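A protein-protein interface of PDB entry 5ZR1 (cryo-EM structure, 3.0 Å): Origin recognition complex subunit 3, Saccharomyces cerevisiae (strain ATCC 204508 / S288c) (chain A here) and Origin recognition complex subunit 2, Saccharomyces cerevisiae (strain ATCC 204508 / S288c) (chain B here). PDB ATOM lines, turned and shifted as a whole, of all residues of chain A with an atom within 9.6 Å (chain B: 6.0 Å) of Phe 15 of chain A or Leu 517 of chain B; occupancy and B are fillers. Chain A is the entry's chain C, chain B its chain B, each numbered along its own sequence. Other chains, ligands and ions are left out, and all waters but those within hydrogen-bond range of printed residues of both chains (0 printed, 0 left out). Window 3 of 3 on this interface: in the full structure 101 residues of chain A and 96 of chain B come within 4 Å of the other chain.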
ATOM      1  N   PHE A  15      24.553  15.950 -20.971  1.00  0.00           N
ATOM      2  CA  PHE A  15      25.809  15.398 -21.464  1.00  0.00           C
ATOM      3  C   PHE A  15      25.590  14.179 -22.353  1.00  0.00           C
ATOM      4  O   PHE A  15      25.622  13.044 -21.880  1.00  0.00           O
ATOM      5  CB  PHE A  15      26.722  15.012 -20.301  1.00  0.00           C
ATOM      6  CG  PHE A  15      27.260  16.180 -19.529  1.00  0.00           C
ATOM      7  CD1 PHE A  15      28.271  16.957 -20.057  1.00  0.00           C
ATOM      8  CD2 PHE A  15      26.784  16.477 -18.267  1.00  0.00           C
ATOM      9  CE1 PHE A  15      28.796  18.020 -19.356  1.00  0.00           C
ATOM     10  CE2 PHE A  15      27.299  17.542 -17.557  1.00  0.00           C
ATOM     11  CZ  PHE A  15      28.312  18.315 -18.105  1.00  0.00           C
ATOM     12  N   ALA A  16      25.371  14.418 -23.642  1.00  0.00           N
ATOM     13  CA  ALA A  16      25.195  13.322 -24.577  1.00  0.00           C
ATOM     14  C   ALA A  16      26.536  12.670 -24.896  1.00  0.00           C
ATOM     15  O   ALA A  16      27.600  13.284 -24.786  1.00  0.00           O
ATOM     16  CB  ALA A  16      24.533  13.813 -25.864  1.00  0.00           C
ATOM     17  N   ASP A  17      26.473  11.398 -25.292  1.00  0.00           N
ATOM     18  CA  ASP A  17      27.676  10.704 -25.726  1.00  0.00           C
ATOM     19  C   ASP A  17      28.130  11.152 -27.108  1.00  0.00           C
ATOM     20  O   ASP A  17      29.321  11.056 -27.415  1.00  0.00           O
ATOM     21  CB  ASP A  17      27.451   9.190 -25.679  1.00  0.00           C
ATOM     22  CG  ASP A  17      26.220   8.746 -26.453  1.00  0.00           C
ATOM     23  OD1 ASP A  17      25.495   9.601 -27.002  1.00  0.00           O
ATOM     24  OD2 ASP A  17      25.967   7.525 -26.496  1.00  0.00           O
ATOM     25  N   ALA A  18      27.212  11.670 -27.929  1.00  0.00           N
ATOM     26  CA  ALA A  18      27.554  12.210 -29.239  1.00  0.00           C
ATOM     27  C   ALA A  18      28.446  13.440 -29.155  1.00  0.00           C
ATOM     28  O   ALA A  18      29.163  13.736 -30.114  1.00  0.00           O
ATOM     29  CB  ALA A  18      26.281  12.566 -30.005  1.00  0.00           C
ATOM     30  N   GLN A  19      28.416  14.158 -28.036  1.00  0.00           N
ATOM     31  CA  GLN A  19      29.225  15.351 -27.864  1.00  0.00           C
ATOM     32  C   GLN A  19      30.526  15.070 -27.132  1.00  0.00           C
ATOM     33  O   GLN A  19      31.388  15.950 -27.064  1.00  0.00           O
ATOM     34  CB  GLN A  19      28.431  16.411 -27.100  1.00  0.00           C
ATOM     35  CG  GLN A  19      27.027  16.631 -27.641  1.00  0.00           C
ATOM     36  CD  GLN A  19      27.001  17.063 -29.091  1.00  0.00           C
ATOM     37  OE1 GLN A  19      27.841  17.840 -29.539  1.00  0.00           O
ATOM     38  NE2 GLN A  19      26.022  16.562 -29.834  1.00  0.00           N
ATOM     39  N   ARG A  20      30.681  13.873 -26.581  1.00  0.00           N
ATOM     40  CA  ARG A  20      31.904  13.470 -25.914  1.00  0.00           C
ATOM     41  C   ARG A  20      32.934  13.074 -26.972  1.00  0.00           C
ATOM     42  O   ARG A  20      32.620  12.930 -28.154  1.00  0.00           O
ATOM     43  CB  ARG A  20      31.599  12.319 -24.945  1.00  0.00           C
ATOM     44  CG  ARG A  20      32.651  12.014 -23.876  1.00  0.00           C
ATOM     45  CD  ARG A  20      32.229  10.885 -22.958  1.00  0.00           C
ATOM     46  NE  ARG A  20      31.061  11.239 -22.163  1.00  0.00           N
ATOM     47  CZ  ARG A  20      29.879  10.644 -22.264  1.00  0.00           C
ATOM     48  NH1 ARG A  20      29.704   9.651 -23.123  1.00  0.00           N
ATOM     49  NH2 ARG A  20      28.873  11.039 -21.497  1.00  0.00           N
ATOM     50  N   TYR A  23      34.000   7.584 -26.245  1.00  0.00           N
ATOM     51  CA  TYR A  23      33.240   6.810 -25.278  1.00  0.00           C
ATOM     52  C   TYR A  23      33.146   5.352 -25.713  1.00  0.00           C
ATOM     53  O   TYR A  23      33.376   5.007 -26.871  1.00  0.00           O
ATOM     54  CB  TYR A  23      31.852   7.406 -25.054  1.00  0.00           C
ATOM     55  CG  TYR A  23      30.856   7.273 -26.175  1.00  0.00           C
ATOM     56  CD1 TYR A  23      30.828   8.180 -27.221  1.00  0.00           C
ATOM     57  CD2 TYR A  23      29.884   6.286 -26.139  1.00  0.00           C
ATOM     58  CE1 TYR A  23      29.894   8.072 -28.226  1.00  0.00           C
ATOM     59  CE2 TYR A  23      28.948   6.174 -27.134  1.00  0.00           C
ATOM     60  CZ  TYR A  23      28.951   7.070 -28.171  1.00  0.00           C
ATOM     61  OH  TYR A  23      28.006   6.953 -29.163  1.00  0.00           O
ATOM     62  N   VAL B 513      27.081  22.565 -24.972  1.00  0.00           N
ATOM     63  CA  VAL B 513      26.992  21.728 -23.782  1.00  0.00           C
ATOM     64  C   VAL B 513      26.312  22.486 -22.645  1.00  0.00           C
ATOM     65  O   VAL B 513      25.512  21.910 -21.898  1.00  0.00           O
ATOM     66  CB  VAL B 513      28.391  21.214 -23.388  1.00  0.00           C
ATOM     67  CG1 VAL B 513      28.333  20.360 -22.133  1.00  0.00           C
ATOM     68  CG2 VAL B 513      28.988  20.408 -24.521  1.00  0.00           C
ATOM     69  N   LEU B 514      26.573  23.797 -22.530  1.00  0.00           N
ATOM     70  CA  LEU B 514      25.965  24.604 -21.473  1.00  0.00           C
ATOM     71  C   LEU B 514      24.451  24.728 -21.596  1.00  0.00           C
ATOM     72  O   LEU B 514      23.791  25.012 -20.594  1.00  0.00           O
ATOM     73  CB  LEU B 514      26.524  26.030 -21.440  1.00  0.00           C
ATOM     74  CG  LEU B 514      27.739  26.515 -20.640  1.00  0.00           C
ATOM     75  CD1 LEU B 514      27.661  26.082 -19.180  1.00  0.00           C
ATOM     76  CD2 LEU B 514      29.064  26.181 -21.255  1.00  0.00           C
ATOM     77  N   GLN B 515      23.890  24.537 -22.794  1.00  0.00           N
ATOM     78  CA  GLN B 515      22.479  24.844 -23.007  1.00  0.00           C
ATOM     79  C   GLN B 515      21.556  23.860 -22.299  1.00  0.00           C
ATOM     80  O   GLN B 515      20.430  24.221 -21.943  1.00  0.00           O
ATOM     81  CB  GLN B 515      22.166  24.867 -24.501  1.00  0.00           C
ATOM     82  CG  GLN B 515      22.826  25.996 -25.258  1.00  0.00           C
ATOM     83  CD  GLN B 515      22.493  25.965 -26.733  1.00  0.00           C
ATOM     84  OE1 GLN B 515      21.801  25.062 -27.203  1.00  0.00           O
ATOM     85  NE2 GLN B 515      22.987  26.949 -27.473  1.00  0.00           N
ATOM     86  N   SER B 516      22.002  22.626 -22.085  1.00  0.00           N
ATOM     87  CA  SER B 516      21.226  21.637 -21.341  1.00  0.00           C
ATOM     88  C   SER B 516      22.081  21.128 -20.188  1.00  0.00           C
ATOM     89  O   SER B 516      22.682  20.055 -20.274  1.00  0.00           O
ATOM     90  CB  SER B 516      20.775  20.496 -22.255  1.00  0.00           C
ATOM     91  OG  SER B 516      20.086  19.499 -21.519  1.00  0.00           O
ATOM     92  N   LEU B 517      22.102  21.887 -19.096  1.00  0.00           N
ATOM     93  CA  LEU B 517      22.776  21.483 -17.870  1.00  0.00           C
ATOM     94  C   LEU B 517      21.857  21.784 -16.697  1.00  0.00           C
ATOM     95  O   LEU B 517      20.679  22.110 -16.868  1.00  0.00           O
ATOM     96  CB  LEU B 517      24.120  22.199 -17.676  1.00  0.00           C
ATOM     97  CG  LEU B 517      25.269  21.932 -18.636  1.00  0.00           C
ATOM     98  CD1 LEU B 517      26.502  22.690 -18.208  1.00  0.00           C
ATOM     99  CD2 LEU B 517      25.548  20.464 -18.713  1.00  0.00           C
ATOM    100  N   THR B 518      22.412  21.677 -15.499  1.00  0.00           N
ATOM    101  CA  THR B 518      21.748  22.121 -14.288  1.00  0.00           C
ATOM    102  C   THR B 518      22.071  23.599 -14.089  1.00  0.00           C
ATOM    103  O   THR B 518      23.121  24.079 -14.526  1.00  0.00           O
ATOM    104  CB  THR B 518      22.227  21.280 -13.099  1.00  0.00           C
ATOM    105  OG1 THR B 518      22.188  19.896 -13.465  1.00  0.00           O
ATOM    106  CG2 THR B 518      21.322  21.453 -11.882  1.00  0.00           C
ATOM    107  N   VAL B 519      21.146  24.330 -13.460  1.00  0.00           N
ATOM    108  CA  VAL B 519      21.416  25.726 -13.125  1.00  0.00           C
ATOM    109  C   VAL B 519      22.522  25.832 -12.080  1.00  0.00           C
ATOM    110  O   VAL B 519      23.266  26.818 -12.056  1.00  0.00           O
ATOM    111  CB  VAL B 519      20.128  26.439 -12.667  1.00  0.00           C
ATOM    112  CG1 VAL B 519      19.150  26.554 -13.821  1.00  0.00           C
ATOM    113  CG2 VAL B 519      19.472  25.701 -11.503  1.00  0.00           C
ATOM    114  N   SER B 521      25.046  23.750 -11.998  1.00  0.00           N
ATOM    115  CA  SER B 521      26.257  23.452 -12.745  1.00  0.00           C
ATOM    116  C   SER B 521      26.642  24.566 -13.704  1.00  0.00           C
ATOM    117  O   SER B 521      27.803  24.627 -14.124  1.00  0.00           O
ATOM    118  CB  SER B 521      26.093  22.147 -13.526  1.00  0.00           C
ATOM    119  OG  SER B 521      25.908  21.051 -12.649  1.00  0.00           O
ATOM    120  N   LYS B 522      25.703  25.441 -14.064  1.00  0.00           N
ATOM    121  CA  LYS B 522      26.062  26.610 -14.854  1.00  0.00           C
ATOM    122  C   LYS B 522      26.520  27.766 -13.982  1.00  0.00           C
ATOM    123  O   LYS B 522      27.343  28.573 -14.423  1.00  0.00           O
ATOM    124  CB  LYS B 522      24.893  27.057 -15.730  1.00  0.00           C
ATOM    125  CG  LYS B 522      24.577  26.116 -16.867  1.00  0.00           C
ATOM    126  CD  LYS B 522      23.662  26.782 -17.879  1.00  0.00           C
ATOM    127  CE  LYS B 522      22.226  26.864 -17.410  1.00  0.00           C
ATOM    128  NZ  LYS B 522      21.353  27.418 -18.481  1.00  0.00           N
ATOM    129  N   GLU B 581      32.346  16.263 -14.725  1.00  0.00           N
ATOM    130  CA  GLU B 581      31.516  16.270 -15.920  1.00  0.00           C
ATOM    131  C   GLU B 581      32.002  17.299 -16.937  1.00  0.00           C
ATOM    132  O   GLU B 581      31.746  17.149 -18.135  1.00  0.00           O
ATOM    133  CB  GLU B 581      30.062  16.518 -15.516  1.00  0.00           C
ATOM    134  CG  GLU B 581      29.816  17.864 -14.849  1.00  0.00           C
ATOM    135  CD  GLU B 581      28.404  18.015 -14.319  1.00  0.00           C
ATOM    136  OE1 GLU B 581      27.629  17.041 -14.402  1.00  0.00           O
ATOM    137  OE2 GLU B 581      28.066  19.112 -13.826  1.00  0.00           O
ATOM    138  N   PHE B 582      32.701  18.345 -16.481  1.00  0.00           N
ATOM    139  CA  PHE B 582      33.372  19.267 -17.393  1.00  0.00           C
ATOM    140  C   PHE B 582      34.736  18.741 -17.820  1.00  0.00           C
ATOM    141  O   PHE B 582      35.197  19.057 -18.921  1.00  0.00           O
ATOM    142  CB  PHE B 582      33.540  20.642 -16.740  1.00  0.00           C
ATOM    143  CG  PHE B 582      32.252  21.375 -16.509  1.00  0.00           C
ATOM    144  CD1 PHE B 582      31.662  22.098 -17.529  1.00  0.00           C
ATOM    145  CD2 PHE B 582      31.637  21.354 -15.268  1.00  0.00           C
ATOM    146  CE1 PHE B 582      30.478  22.783 -17.322  1.00  0.00           C
ATOM    147  CE2 PHE B 582      30.451  22.037 -15.055  1.00  0.00           C
ATOM    148  CZ  PHE B 582      29.874  22.751 -16.083  1.00  0.00           C
ATOM    149  N   GLU B 584      35.556  15.463 -18.273  1.00  0.00           N
ATOM    150  CA  GLU B 584      35.336  14.425 -19.278  1.00  0.00           C
ATOM    151  C   GLU B 584      34.970  14.998 -20.645  1.00  0.00           C
ATOM    152  O   GLU B 584      35.216  14.343 -21.663  1.00  0.00           O
ATOM    153  CB  GLU B 584      34.258  13.444 -18.808  1.00  0.00           C
ATOM    154  CG  GLU B 584      32.868  14.032 -18.661  1.00  0.00           C
ATOM    155  CD  GLU B 584      31.859  13.017 -18.160  1.00  0.00           C
ATOM    156  OE1 GLU B 584      32.252  11.857 -17.923  1.00  0.00           O
ATOM    157  OE2 GLU B 584      30.676  13.382 -17.997  1.00  0.00           O
ATOM    158  N   HIS B 585      34.401  16.200 -20.687  1.00  0.00           N
ATOM    159  CA  HIS B 585      34.158  16.929 -21.921  1.00  0.00           C
ATOM    160  C   HIS B 585      35.227  17.968 -22.212  1.00  0.00           C
ATOM    161  O   HIS B 585      35.116  18.683 -23.214  1.00  0.00           O
ATOM    162  CB  HIS B 585      32.781  17.582 -21.857  1.00  0.00           C
ATOM    163  CG  HIS B 585      31.664  16.618 -22.085  1.00  0.00           C
ATOM    164  ND1 HIS B 585      31.112  16.404 -23.328  1.00  0.00           N
ATOM    165  CD2 HIS B 585      31.087  15.717 -21.258  1.00  0.00           C
ATOM    166  CE1 HIS B 585      30.179  15.474 -23.239  1.00  0.00           C
ATOM    167  NE2 HIS B 585      30.146  15.038 -21.992  1.00  0.00           N
ATOM    168  N   MET B 587      36.041  20.800 -21.002  1.00  0.00           N
ATOM    169  CA  MET B 587      35.683  22.198 -20.853  1.00  0.00           C
ATOM    170  C   MET B 587      36.407  22.851 -19.690  1.00  0.00           C
ATOM    171  O   MET B 587      36.363  24.076 -19.550  1.00  0.00           O
ATOM    172  CB  MET B 587      34.181  22.306 -20.643  1.00  0.00           C
ATOM    173  CG  MET B 587      33.380  21.842 -21.830  1.00  0.00           C
ATOM    174  SD  MET B 587      31.671  21.662 -21.346  1.00  0.00           S
ATOM    175  CE  MET B 587      31.333  23.351 -20.930  1.00  0.00           C
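Leu 517 of chain B touches just one residue of chain A: Phe 15. Leu 514 of chain B touches none of the printed residues of chain A. No residue of chain A comes within 4 Å of Ser 516 of chain B. Thr 518 of chain B touches none of the printed residues of chain A. Printed residues of chain B within 4 Å of Gln 19 of chain A: His 585 (3.8 Å). Of the printed residues of chain B, Ala 16 of chain A touches His 585. Printed residues of chain A within 4 Å of His 585 of chain B: Phe 15 (3.3 Å), Ala 16 (3.7 Å), Gln 19 (3.8 Å) and Arg 20 (3.7 Å). Of the printed residues of chain A, Val 513 of chain B touches Phe 15. Gln 515 of chain B touches none of the printed residues of chain A.
OG of Ser 521 of chain B sits at hydrogen-bond distance from OE2 of Glu 581 of chain B (3.1 Å).
Printed residues of chain A that touch a printed residue of chain B: Phe 15, Ala 16, Gln 19 and Arg 20. Hydrophobic or aromatic side chains of chain A that line the printed part of chain B: Phe 15. Along chain A the printed residues that touch a printed residue of chain B span positions 15 to 20. Printed residues of chain B that touch a printed residue of chain A: Val 513, Leu 517, Glu 581 and His 585. Hydrophobic or aromatic side chains of chain B within 4 Å of the printed part of chain A: Val 513, Leu 517 and His 585. Among the printed residues, no Asp or Glu carboxylate lies within 4 Å of a Lys or Arg side-chain nitrogen of the other chain.
Among the printed residues, merely in contact across the chains: Phe 15 of chain A with Val 513 of chain B, Phe 15 of chain A with Leu 517 of chain B, Phe 15 of chain A with Glu 581 of chain B, Phe 15 of chain A with His 585 of chain B, Ala 16 of chain A with His 585 of chain B, Gln 19 of chain A with His 585 of chain B and Arg 20 of chain A with His 585 of chain B.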
